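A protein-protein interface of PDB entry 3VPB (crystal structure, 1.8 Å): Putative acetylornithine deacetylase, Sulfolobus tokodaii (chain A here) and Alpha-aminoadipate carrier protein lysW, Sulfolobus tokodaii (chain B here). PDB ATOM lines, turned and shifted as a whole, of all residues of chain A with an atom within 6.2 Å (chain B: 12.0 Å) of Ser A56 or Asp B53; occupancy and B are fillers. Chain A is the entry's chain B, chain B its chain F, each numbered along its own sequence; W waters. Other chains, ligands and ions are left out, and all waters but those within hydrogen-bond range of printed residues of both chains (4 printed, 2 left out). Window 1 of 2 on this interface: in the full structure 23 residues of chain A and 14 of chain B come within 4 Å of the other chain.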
ATOM      1  N   ASP A   8      18.165   8.891 -30.428  1.00  0.00           N
ATOM      2  CA  ASP A   8      18.713   7.842 -29.561  1.00  0.00           C
ATOM      3  C   ASP A   8      18.287   8.069 -28.116  1.00  0.00           C
ATOM      4  O   ASP A   8      17.681   7.196 -27.477  1.00  0.00           O
ATOM      5  CB  ASP A   8      20.241   7.617 -29.735  1.00  0.00           C
ATOM      6  CG  ASP A   8      21.085   8.886 -29.585  1.00  0.00           C
ATOM      7  OD1 ASP A   8      22.316   8.819 -29.895  1.00  0.00           O
ATOM      8  OD2 ASP A   8      20.573   9.940 -29.155  1.00  0.00           O
ATOM      9  N   ARG A  53      18.211  13.627 -35.105  1.00  0.00           N
ATOM     10  CA  ARG A  53      18.288  14.109 -33.722  1.00  0.00           C
ATOM     11  C   ARG A  53      19.126  13.284 -32.701  1.00  0.00           C
ATOM     12  O   ARG A  53      19.074  13.591 -31.514  1.00  0.00           O
ATOM     13  CB  ARG A  53      16.858  14.335 -33.186  1.00  0.00           C
ATOM     14  CG  ARG A  53      16.105  15.487 -33.899  1.00  0.00           C
ATOM     15  CD  ARG A  53      16.859  16.805 -33.796  1.00  0.00           C
ATOM     16  NE  ARG A  53      17.044  17.187 -32.390  1.00  0.00           N
ATOM     17  CZ  ARG A  53      17.563  18.348 -32.006  1.00  0.00           C
ATOM     18  NH1 ARG A  53      17.684  18.633 -30.712  1.00  0.00           N
ATOM     19  NH2 ARG A  53      17.934  19.231 -32.924  1.00  0.00           N
ATOM     20  N   PRO A  54      19.905  12.256 -33.134  1.00  0.00           N
ATOM     21  CA  PRO A  54      20.686  11.571 -32.103  1.00  0.00           C
ATOM     22  C   PRO A  54      21.671  12.499 -31.383  1.00  0.00           C
ATOM     23  O   PRO A  54      22.244  13.411 -32.002  1.00  0.00           O
ATOM     24  CB  PRO A  54      21.476  10.507 -32.912  1.00  0.00           C
ATOM     25  CG  PRO A  54      20.625  10.270 -34.107  1.00  0.00           C
ATOM     26  CD  PRO A  54      20.163  11.662 -34.451  1.00  0.00           C
ATOM     27  N   VAL A  55      21.883  12.212 -30.096  1.00  0.00           N
ATOM     28  CA  VAL A  55      22.830  12.940 -29.241  1.00  0.00           C
ATOM     29  C   VAL A  55      24.247  12.517 -29.631  1.00  0.00           C
ATOM     30  O   VAL A  55      25.198  13.309 -29.548  1.00  0.00           O
ATOM     31  CB  VAL A  55      22.592  12.625 -27.735  1.00  0.00           C
ATOM     32  CG1 VAL A  55      23.481  13.500 -26.820  1.00  0.00           C
ATOM     33  CG2 VAL A  55      21.106  12.769 -27.360  1.00  0.00           C
ATOM     34  N   SER A  56      24.399  11.263 -30.065  1.00  0.00           N
ATOM     35  CA  SER A  56      25.721  10.774 -30.511  1.00  0.00           C
ATOM     36  C   SER A  56      25.951  11.341 -31.904  1.00  0.00           C
ATOM     37  O   SER A  56      25.130  11.107 -32.786  1.00  0.00           O
ATOM     38  CB  SER A  56      25.723   9.249 -30.606  1.00  0.00           C
ATOM     39  OG  SER A  56      26.818   8.807 -31.406  1.00  0.00           O
ATOM     40  N   MET A  57      27.034  12.083 -32.101  1.00  0.00           N
ATOM     41  CA  MET A  57      27.340  12.629 -33.425  1.00  0.00           C
ATOM     42  C   MET A  57      27.558  11.507 -34.466  1.00  0.00           C
ATOM     43  O   MET A  57      27.113  11.627 -35.601  1.00  0.00           O
ATOM     44  CB  MET A  57      28.548  13.548 -33.388  1.00  0.00           C
ATOM     45  CG  MET A  57      28.841  14.201 -34.745  1.00  0.00           C
ATOM     46  SD  MET A  57      29.982  13.202 -35.715  1.00  0.00           S
ATOM     47  CE  MET A  57      31.479  13.870 -34.959  1.00  0.00           C
ATOM     48  N   TYR A  58      28.202  10.416 -34.076  1.00  0.00           N
ATOM     49  CA  TYR A  58      28.387   9.304 -35.030  1.00  0.00           C
ATOM     50  C   TYR A  58      27.058   8.669 -35.442  1.00  0.00           C
ATOM     51  O   TYR A  58      26.861   8.352 -36.623  1.00  0.00           O
ATOM     52  CB  TYR A  58      29.363   8.257 -34.503  1.00  0.00           C
ATOM     53  CG  TYR A  58      30.794   8.766 -34.405  1.00  0.00           C
ATOM     54  CD1 TYR A  58      31.470   9.254 -35.523  1.00  0.00           C
ATOM     55  CD2 TYR A  58      31.473   8.735 -33.195  1.00  0.00           C
ATOM     56  CE1 TYR A  58      32.791   9.732 -35.415  1.00  0.00           C
ATOM     57  CE2 TYR A  58      32.782   9.197 -33.084  1.00  0.00           C
ATOM     58  CZ  TYR A  58      33.433   9.678 -34.192  1.00  0.00           C
ATOM     59  OH  TYR A  58      34.732  10.128 -34.052  1.00  0.00           O
ATOM     60  N   ARG A  59      26.145   8.504 -34.487  1.00  0.00           N
ATOM     61  CA  ARG A  59      24.782   8.031 -34.808  1.00  0.00           C
ATOM     62  C   ARG A  59      24.046   8.994 -35.728  1.00  0.00           C
ATOM     63  O   ARG A  59      23.369   8.559 -36.656  1.00  0.00           O
ATOM     64  CB  ARG A  59      23.940   7.786 -33.555  1.00  0.00           C
ATOM     65  CG  ARG A  59      24.408   6.600 -32.734  1.00  0.00           C
ATOM     66  CD  ARG A  59      23.298   6.096 -31.839  1.00  0.00           C
ATOM     67  NE  ARG A  59      23.781   4.982 -31.029  1.00  0.00           N
ATOM     68  CZ  ARG A  59      23.861   5.013 -29.703  1.00  0.00           C
ATOM     69  NH1 ARG A  59      24.306   3.948 -29.059  1.00  0.00           N
ATOM     70  NH2 ARG A  59      23.448   6.092 -29.016  1.00  0.00           N
ATOM     71  N   ALA A  60      24.200  10.304 -35.500  1.00  0.00           N
ATOM     72  CA  ALA A  60      23.609  11.292 -36.384  1.00  0.00           C
ATOM     73  C   ALA A  60      24.199  11.182 -37.792  1.00  0.00           C
ATOM     74  O   ALA A  60      23.459  11.199 -38.793  1.00  0.00           O
ATOM     75  CB  ALA A  60      23.811  12.734 -35.810  1.00  0.00           C
ATOM     76  N   LEU A  61      25.526  11.109 -37.868  1.00  0.00           N
ATOM     77  CA  LEU A  61      26.226  11.004 -39.148  1.00  0.00           C
ATOM     78  C   LEU A  61      25.796   9.771 -39.929  1.00  0.00           C
ATOM     79  O   LEU A  61      25.435   9.855 -41.108  1.00  0.00           O
ATOM     80  CB  LEU A  61      27.745  10.990 -38.931  1.00  0.00           C
ATOM     81  CG  LEU A  61      28.607  10.889 -40.177  1.00  0.00           C
ATOM     82  CD1 LEU A  61      28.373  12.097 -41.173  1.00  0.00           C
ATOM     83  CD2 LEU A  61      30.060  10.780 -39.804  1.00  0.00           C
ATOM     84  N   ILE A 130      36.517  17.236 -32.038  1.00  0.00           N
ATOM     85  CA  ILE A 130      35.226  16.646 -31.726  1.00  0.00           C
ATOM     86  C   ILE A 130      34.917  16.855 -30.268  1.00  0.00           C
ATOM     87  O   ILE A 130      35.822  16.945 -29.428  1.00  0.00           O
ATOM     88  CB  ILE A 130      35.123  15.141 -32.093  1.00  0.00           C
ATOM     89  CG1 ILE A 130      36.360  14.362 -31.616  1.00  0.00           C
ATOM     90  CG2 ILE A 130      34.894  14.979 -33.583  1.00  0.00           C
ATOM     91  CD1 ILE A 130      36.238  12.856 -31.839  1.00  0.00           C
ATOM     92  N   GLY A 131      33.629  16.977 -29.984  1.00  0.00           N
ATOM     93  CA  GLY A 131      33.159  17.193 -28.645  1.00  0.00           C
ATOM     94  C   GLY A 131      32.093  18.263 -28.663  1.00  0.00           C
ATOM     95  O   GLY A 131      31.910  18.976 -29.672  1.00  0.00           O
ATOM     96  N   SER A 132      31.386  18.357 -27.549  1.00  0.00           N
ATOM     97  CA  SER A 132      30.332  19.323 -27.358  1.00  0.00           C
ATOM     98  C   SER A 132      30.253  19.537 -25.861  1.00  0.00           C
ATOM     99  O   SER A 132      30.986  18.890 -25.108  1.00  0.00           O
ATOM    100  CB  SER A 132      29.024  18.742 -27.912  1.00  0.00           C
ATOM    101  OG  SER A 132      27.962  19.657 -27.808  1.00  0.00           O
ATOM    102  N   ARG A 135      33.298  19.928 -23.429  1.00  0.00           N
ATOM    103  CA  ARG A 135      34.109  18.780 -23.034  1.00  0.00           C
ATOM    104  C   ARG A 135      35.547  18.883 -23.602  1.00  0.00           C
ATOM    105  O   ARG A 135      35.716  19.053 -24.816  1.00  0.00           O
ATOM    106  CB  ARG A 135      33.436  17.479 -23.516  1.00  0.00           C
ATOM    107  CG  ARG A 135      33.829  16.242 -22.740  1.00  0.00           C
ATOM    108  CD  ARG A 135      32.834  15.094 -22.979  1.00  0.00           C
ATOM    109  NE  ARG A 135      32.589  14.917 -24.414  1.00  0.00           N
ATOM    110  CZ  ARG A 135      31.423  15.134 -25.012  1.00  0.00           C
ATOM    111  NH1 ARG A 135      30.370  15.541 -24.306  1.00  0.00           N
ATOM    112  NH2 ARG A 135      31.322  14.975 -26.325  1.00  0.00           N
ATOM    113  N   ASN A 158      39.851   7.831 -28.611  1.00  0.00           N
ATOM    114  CA  ASN A 158      39.475   8.281 -29.966  1.00  0.00           C
ATOM    115  C   ASN A 158      40.617   9.172 -30.475  1.00  0.00           C
ATOM    116  O   ASN A 158      40.870  10.253 -29.935  1.00  0.00           O
ATOM    117  CB  ASN A 158      38.146   9.039 -29.918  1.00  0.00           C
ATOM    118  CG  ASN A 158      37.682   9.503 -31.291  1.00  0.00           C
ATOM    119  OD1 ASN A 158      38.494   9.787 -32.160  1.00  0.00           O
ATOM    120  ND2 ASN A 158      36.363   9.556 -31.490  1.00  0.00           N
ATOM    121  N   VAL A 254      23.310  19.175 -34.601  1.00  0.00           N
ATOM    122  CA  VAL A 254      22.104  18.691 -33.905  1.00  0.00           C
ATOM    123  C   VAL A 254      21.809  19.647 -32.752  1.00  0.00           C
ATOM    124  O   VAL A 254      22.070  19.343 -31.570  1.00  0.00           O
ATOM    125  CB  VAL A 254      22.219  17.232 -33.392  1.00  0.00           C
ATOM    126  CG1 VAL A 254      20.856  16.751 -32.831  1.00  0.00           C
ATOM    127  CG2 VAL A 254      22.648  16.260 -34.523  1.00  0.00           C
ATOM    128  N   GLY B  22      12.689   6.316 -24.787  1.00  0.00           N
ATOM    129  CA  GLY B  22      13.960   7.012 -25.068  1.00  0.00           C
ATOM    130  C   GLY B  22      14.339   8.117 -24.083  1.00  0.00           C
ATOM    131  O   GLY B  22      15.488   8.563 -24.054  1.00  0.00           O
ATOM    132  N   ILE B  24      15.201   9.840 -20.439  1.00  0.00           N
ATOM    133  CA  ILE B  24      16.047   9.444 -19.320  1.00  0.00           C
ATOM    134  C   ILE B  24      15.372   9.798 -18.008  1.00  0.00           C
ATOM    135  O   ILE B  24      14.737  10.859 -17.897  1.00  0.00           O
ATOM    136  CB  ILE B  24      17.442  10.128 -19.419  1.00  0.00           C
ATOM    137  CG1 ILE B  24      18.128   9.765 -20.738  1.00  0.00           C
ATOM    138  CG2 ILE B  24      18.348   9.744 -18.247  1.00  0.00           C
ATOM    139  CD1 ILE B  24      18.365   8.259 -20.949  1.00  0.00           C
ATOM    140  N   GLU B  34      16.748   4.537 -18.833  1.00  0.00           N
ATOM    141  CA  GLU B  34      16.115   5.003 -20.071  1.00  0.00           C
ATOM    142  C   GLU B  34      14.784   4.280 -20.229  1.00  0.00           C
ATOM    143  O   GLU B  34      14.722   3.074 -20.031  1.00  0.00           O
ATOM    144  CB  GLU B  34      17.010   4.725 -21.288  1.00  0.00           C
ATOM    145  CG  GLU B  34      16.509   5.396 -22.617  1.00  0.00           C
ATOM    146  CD  GLU B  34      17.645   5.874 -23.542  1.00  0.00           C
ATOM    147  OE1 GLU B  34      17.344   6.385 -24.651  1.00  0.00           O
ATOM    148  OE2 GLU B  34      18.832   5.760 -23.168  1.00  0.00           O
ATOM    149  N   GLU B  48      22.697   4.668 -21.338  1.00  0.00           N
ATOM    150  CA  GLU B  48      24.059   4.755 -21.872  1.00  0.00           C
ATOM    151  C   GLU B  48      24.859   5.828 -21.157  1.00  0.00           C
ATOM    152  O   GLU B  48      24.308   6.848 -20.727  1.00  0.00           O
ATOM    153  CB  GLU B  48      24.018   5.087 -23.369  1.00  0.00           C
ATOM    154  CG  GLU B  48      23.711   3.906 -24.250  1.00  0.00           C
ATOM    155  CD  GLU B  48      24.129   4.151 -25.697  1.00  0.00           C
ATOM    156  OE1 GLU B  48      24.038   5.315 -26.171  1.00  0.00           O
ATOM    157  OE2 GLU B  48      24.550   3.170 -26.352  1.00  0.00           O
ATOM    158  N   GLN B  49      26.161   5.600 -21.021  1.00  0.00           N
ATOM    159  CA  GLN B  49      27.049   6.613 -20.468  1.00  0.00           C
ATOM    160  C   GLN B  49      27.469   7.575 -21.568  1.00  0.00           C
ATOM    161  O   GLN B  49      27.428   7.222 -22.740  1.00  0.00           O
ATOM    162  CB  GLN B  49      28.251   5.956 -19.787  1.00  0.00           C
ATOM    163  CG  GLN B  49      27.897   5.455 -18.391  1.00  0.00           C
ATOM    164  CD  GLN B  49      28.818   4.358 -17.884  1.00  0.00           C
ATOM    165  OE1 GLN B  49      30.030   4.377 -18.132  1.00  0.00           O
ATOM    166  NE2 GLN B  49      28.244   3.394 -17.152  1.00  0.00           N
ATOM    167  N   VAL B  50      27.828   8.798 -21.185  1.00  0.00           N
ATOM    168  CA  VAL B  50      28.165   9.843 -22.139  1.00  0.00           C
ATOM    169  C   VAL B  50      29.385   9.422 -22.967  1.00  0.00           C
ATOM    170  O   VAL B  50      30.424   9.048 -22.409  1.00  0.00           O
ATOM    171  CB  VAL B  50      28.411  11.200 -21.439  1.00  0.00           C
ATOM    172  CG1 VAL B  50      28.711  12.286 -22.444  1.00  0.00           C
ATOM    173  CG2 VAL B  50      27.187  11.600 -20.606  1.00  0.00           C
ATOM    174  N   GLY B  51      29.235   9.474 -24.289  1.00  0.00           N
ATOM    175  CA  GLY B  51      30.327   9.165 -25.221  1.00  0.00           C
ATOM    176  C   GLY B  51      31.119  10.411 -25.568  1.00  0.00           C
ATOM    177  O   GLY B  51      30.666  11.535 -25.350  1.00  0.00           O
ATOM    178  N   GLU B  52      32.309  10.210 -26.134  1.00  0.00           N
ATOM    179  CA  GLU B  52      33.184  11.333 -26.458  1.00  0.00           C
ATOM    180  C   GLU B  52      32.637  12.169 -27.617  1.00  0.00           C
ATOM    181  O   GLU B  52      33.055  13.324 -27.797  1.00  0.00           O
ATOM    182  CB  GLU B  52      34.602  10.820 -26.743  1.00  0.00           C
ATOM    183  CG  GLU B  52      34.861  10.357 -28.178  1.00  0.00           C
ATOM    184  CD  GLU B  52      34.328   8.964 -28.504  1.00  0.00           C
ATOM    185  OE1 GLU B  52      33.726   8.304 -27.632  1.00  0.00           O
ATOM    186  OE2 GLU B  52      34.493   8.543 -29.668  1.00  0.00           O
ATOM    187  N   ASP B  53      31.678  11.603 -28.353  1.00  0.00           N
ATOM    188  CA  ASP B  53      31.016  12.296 -29.484  1.00  0.00           C
ATOM    189  C   ASP B  53      29.603  12.827 -29.158  1.00  0.00           C
ATOM    190  O   ASP B  53      28.851  13.267 -30.060  1.00  0.00           O
ATOM    191  CB  ASP B  53      30.924  11.337 -30.680  1.00  0.00           C
ATOM    192  CG  ASP B  53      29.945  10.199 -30.439  1.00  0.00           C
ATOM    193  OD1 ASP B  53      29.902   9.680 -29.297  1.00  0.00           O
ATOM    194  OD2 ASP B  53      29.213   9.825 -31.391  1.00  0.00           O
ATOM    195  N   TRP B  54      29.225  12.788 -27.882  1.00  0.00           N
ATOM    196  CA  TRP B  54      27.891  13.245 -27.486  1.00  0.00           C
ATOM    197  C   TRP B  54      27.748  14.759 -27.442  1.00  0.00           C
ATOM    198  O   TRP B  54      28.631  15.460 -26.935  1.00  0.00           O
ATOM    199  CB  TRP B  54      27.521  12.711 -26.111  1.00  0.00           C
ATOM    200  CG  TRP B  54      27.035  11.313 -26.109  1.00  0.00           C
ATOM    201  CD1 TRP B  54      27.408  10.294 -26.957  1.00  0.00           C
ATOM    202  CD2 TRP B  54      26.069  10.764 -25.216  1.00  0.00           C
ATOM    203  NE1 TRP B  54      26.734   9.141 -26.630  1.00  0.00           N
ATOM    204  CE2 TRP B  54      25.905   9.399 -25.567  1.00  0.00           C
ATOM    205  CE3 TRP B  54      25.323  11.288 -24.149  1.00  0.00           C
ATOM    206  CZ2 TRP B  54      25.022   8.550 -24.882  1.00  0.00           C
ATOM    207  CZ3 TRP B  54      24.454  10.439 -23.467  1.00  0.00           C
ATOM    208  CH2 TRP B  54      24.310   9.092 -23.847  1.00  0.00           C
ATOM    209  N   GLY B  55      26.601  15.237 -27.918  1.00  0.00           N
ATOM    210  CA  GLY B  55      26.235  16.659 -27.809  1.00  0.00           C
ATOM    211  C   GLY B  55      25.565  17.211 -29.034  1.00  0.00           C
ATOM    212  O   GLY B  55      24.826  16.501 -29.718  1.00  0.00           O
ATOM    213  N   GLU B  56      25.805  18.494 -29.297  1.00  0.00           N
ATOM    214  CA  GLU B  56      25.278  19.169 -30.478  1.00  0.00           C
ATOM    215  C   GLU B  56      26.154  18.947 -31.698  1.00  0.00           C
ATOM    216  O   GLU B  56      25.670  18.966 -32.845  1.00  0.00           O
ATOM    217  CB  GLU B  56      25.222  20.662 -30.241  1.00  0.00           C
ATOM    218  CG  GLU B  56      24.253  21.082 -29.211  1.00  0.00           C
ATOM    219  CD  GLU B  56      23.741  22.471 -29.491  1.00  0.00           C
ATOM    220  OE1 GLU B  56      23.307  23.094 -28.533  1.00  0.00           O
ATOM    221  OE2 GLU B  56      23.768  22.934 -30.667  1.00  0.00           O
ATOM    222  OXT GLU B  56      27.372  18.797 -31.553  1.00  0.00           O
HETATM  223  O   HOH W   1      30.363  15.886 -30.217  1.00  0.00           O
HETATM  224  O   HOH W   2      22.345  17.232 -29.996  1.00  0.00           O
HETATM  225  O   HOH W   3      34.751  14.572 -26.001  1.00  0.00           O
HETATM  226  O   HOH W   4      26.347   6.096 -27.133  1.00  0.00           O
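N of Val A55 sits at hydrogen-bond distance from OD2 of Asp A8 (2.8 Å). The side-chain carboxylate (OD1) of Asp A8 is in hydrogen-bond range of the backbone NH (N) of Ser A56 (3.2 Å). OG of Ser A56 lies close to N of Tyr A58, at 3.4 Å. The backbone NH of Arg A59 sits at hydrogen-bond distance from the side-chain hydroxyl of Ser A56 (3.2 Å). The side-chain hydroxyl of Tyr A58 is in hydrogen-bond range of the side-chain amide nitrogen of Asn A158, at 3.1 Å. The backbone carbonyl oxygen (O) of Ser A132 lies close to the guanidinium group (NH1) of Arg A135.
The backbone NH (N) of Gly B55 lies within hydrogen-bond range of the backbone carbonyl oxygen (O) of Val A55 (2.9 Å). The side-chain hydroxyl (OG) of Ser A56 lies within hydrogen-bond range of the side-chain carboxylate (OD2) of Asp B53, at 2.6 Å. N of Met A57 sits at hydrogen-bond distance from O of Asp B53 (3.0 Å). The side-chain carboxylate of Asp B53 lies within hydrogen-bond range of the backbone NH of Tyr A58 (2.9 Å). OE2 of Glu B48 lies within salt-bridge range of NH1 of Arg A59. The backbone NH of Glu B56 lies within hydrogen-bond range of the side-chain hydroxyl of Ser A132, at 2.9 Å. The guanidinium group (NH2) of Arg A135 is in hydrogen-bond range of the backbone carbonyl oxygen (O) of Glu B52, at 2.8 Å. NH2 of Arg A135 sits at hydrogen-bond distance from O of Trp B54, at 2.8 Å. The side-chain carboxylate (OE2) of Glu B52 is in hydrogen-bond range of the side-chain amide nitrogen (ND2) of Asn A158 (2.8 Å). The chain-end carboxylate (O) of Glu B56 sits at hydrogen-bond distance from the backbone NH (N) of Val A254, 2.9 Å away. O of Asp A8 lies close to OE1 of Glu B34 (3.0 Å).
Ser A56 touches two residues of chain B. Printed residues of chain A within 4 Å of Asp B53: Val A55, Ser A56, Met A57, Tyr A58 and Arg A135. Pro A54 touches none of the printed residues of chain B. Met A57 touches just one residue of chain B: Asp B53 (3.0 Å). Of chain B, only Glu B52 and Asp B53 come within 4 Å of Tyr A58. Of chain B, only Glu B52 comes within 4 Å of Gly A131. Of the printed residues of chain B, Asp A8 touches Glu B34 (3.0 Å). Of the printed residues of chain B, Val A254 touches Glu B56 (2.9 Å). Of the printed residues of chain B, Val A55 touches Asp B53, Trp B54 and Gly B55. Printed residues of chain A within 4 Å of Glu B52: Tyr A58, Gly A131, Arg A135 and Asn A158. The nearest printed residue of chain A that does not touch Asp B53 is Arg A59 (4.6 Å). The nearest printed residue of chain B that does not touch Asn A158 is Asp B53 (5.8 Å).
Water W2 lies within hydrogen-bond range of the backbone carbonyl oxygen of Gly B55 and the backbone carbonyl oxygen of Val A254. Water W4 lies within hydrogen-bond range of OE1 of Glu B48, NE1 of Trp B54 and NH2 of Arg A59. Water W3 bridges the guanidinium group of Arg A135 (2.7 Å) and the backbone carbonyl oxygen of Glu B52 (2.8 Å). Water W1 bridges the backbone carbonyl oxygen of Asp B53 (3.0 Å) and the backbone NH of Gly A131 (3.5 Å).
Among the printed residues, merely in contact across the chains: Val A55 with Trp B54 (3.4 Å), Ser A132 with Trp B54 (3.4 Å), Ser A132 with Gly B55 (3.5 Å), Arg A135 with Gly B51 (3.6 Å), Val A55 with Asp B53 (3.7 Å), Tyr A58 with Glu B52 (3.9 Å), Arg A135 with Asp B53 (3.9 Å), Gly A131 with Glu B52 (3.96 Å) and Ser A56 with Trp B54 (3.96 Å).
Hydrophobic or aromatic side chains of chain B that line the printed part of chain A: Trp B54. Of the 16 printed residues of chain A, 11 touch a printed residue of chain B. Printed residues of chain A that touch a printed residue of chain B: Asp A8, Val A55, Ser A56, Met A57, Tyr A58, Arg A59, Gly A131, Ser A132, Arg A135, Asn A158 and Val A254.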
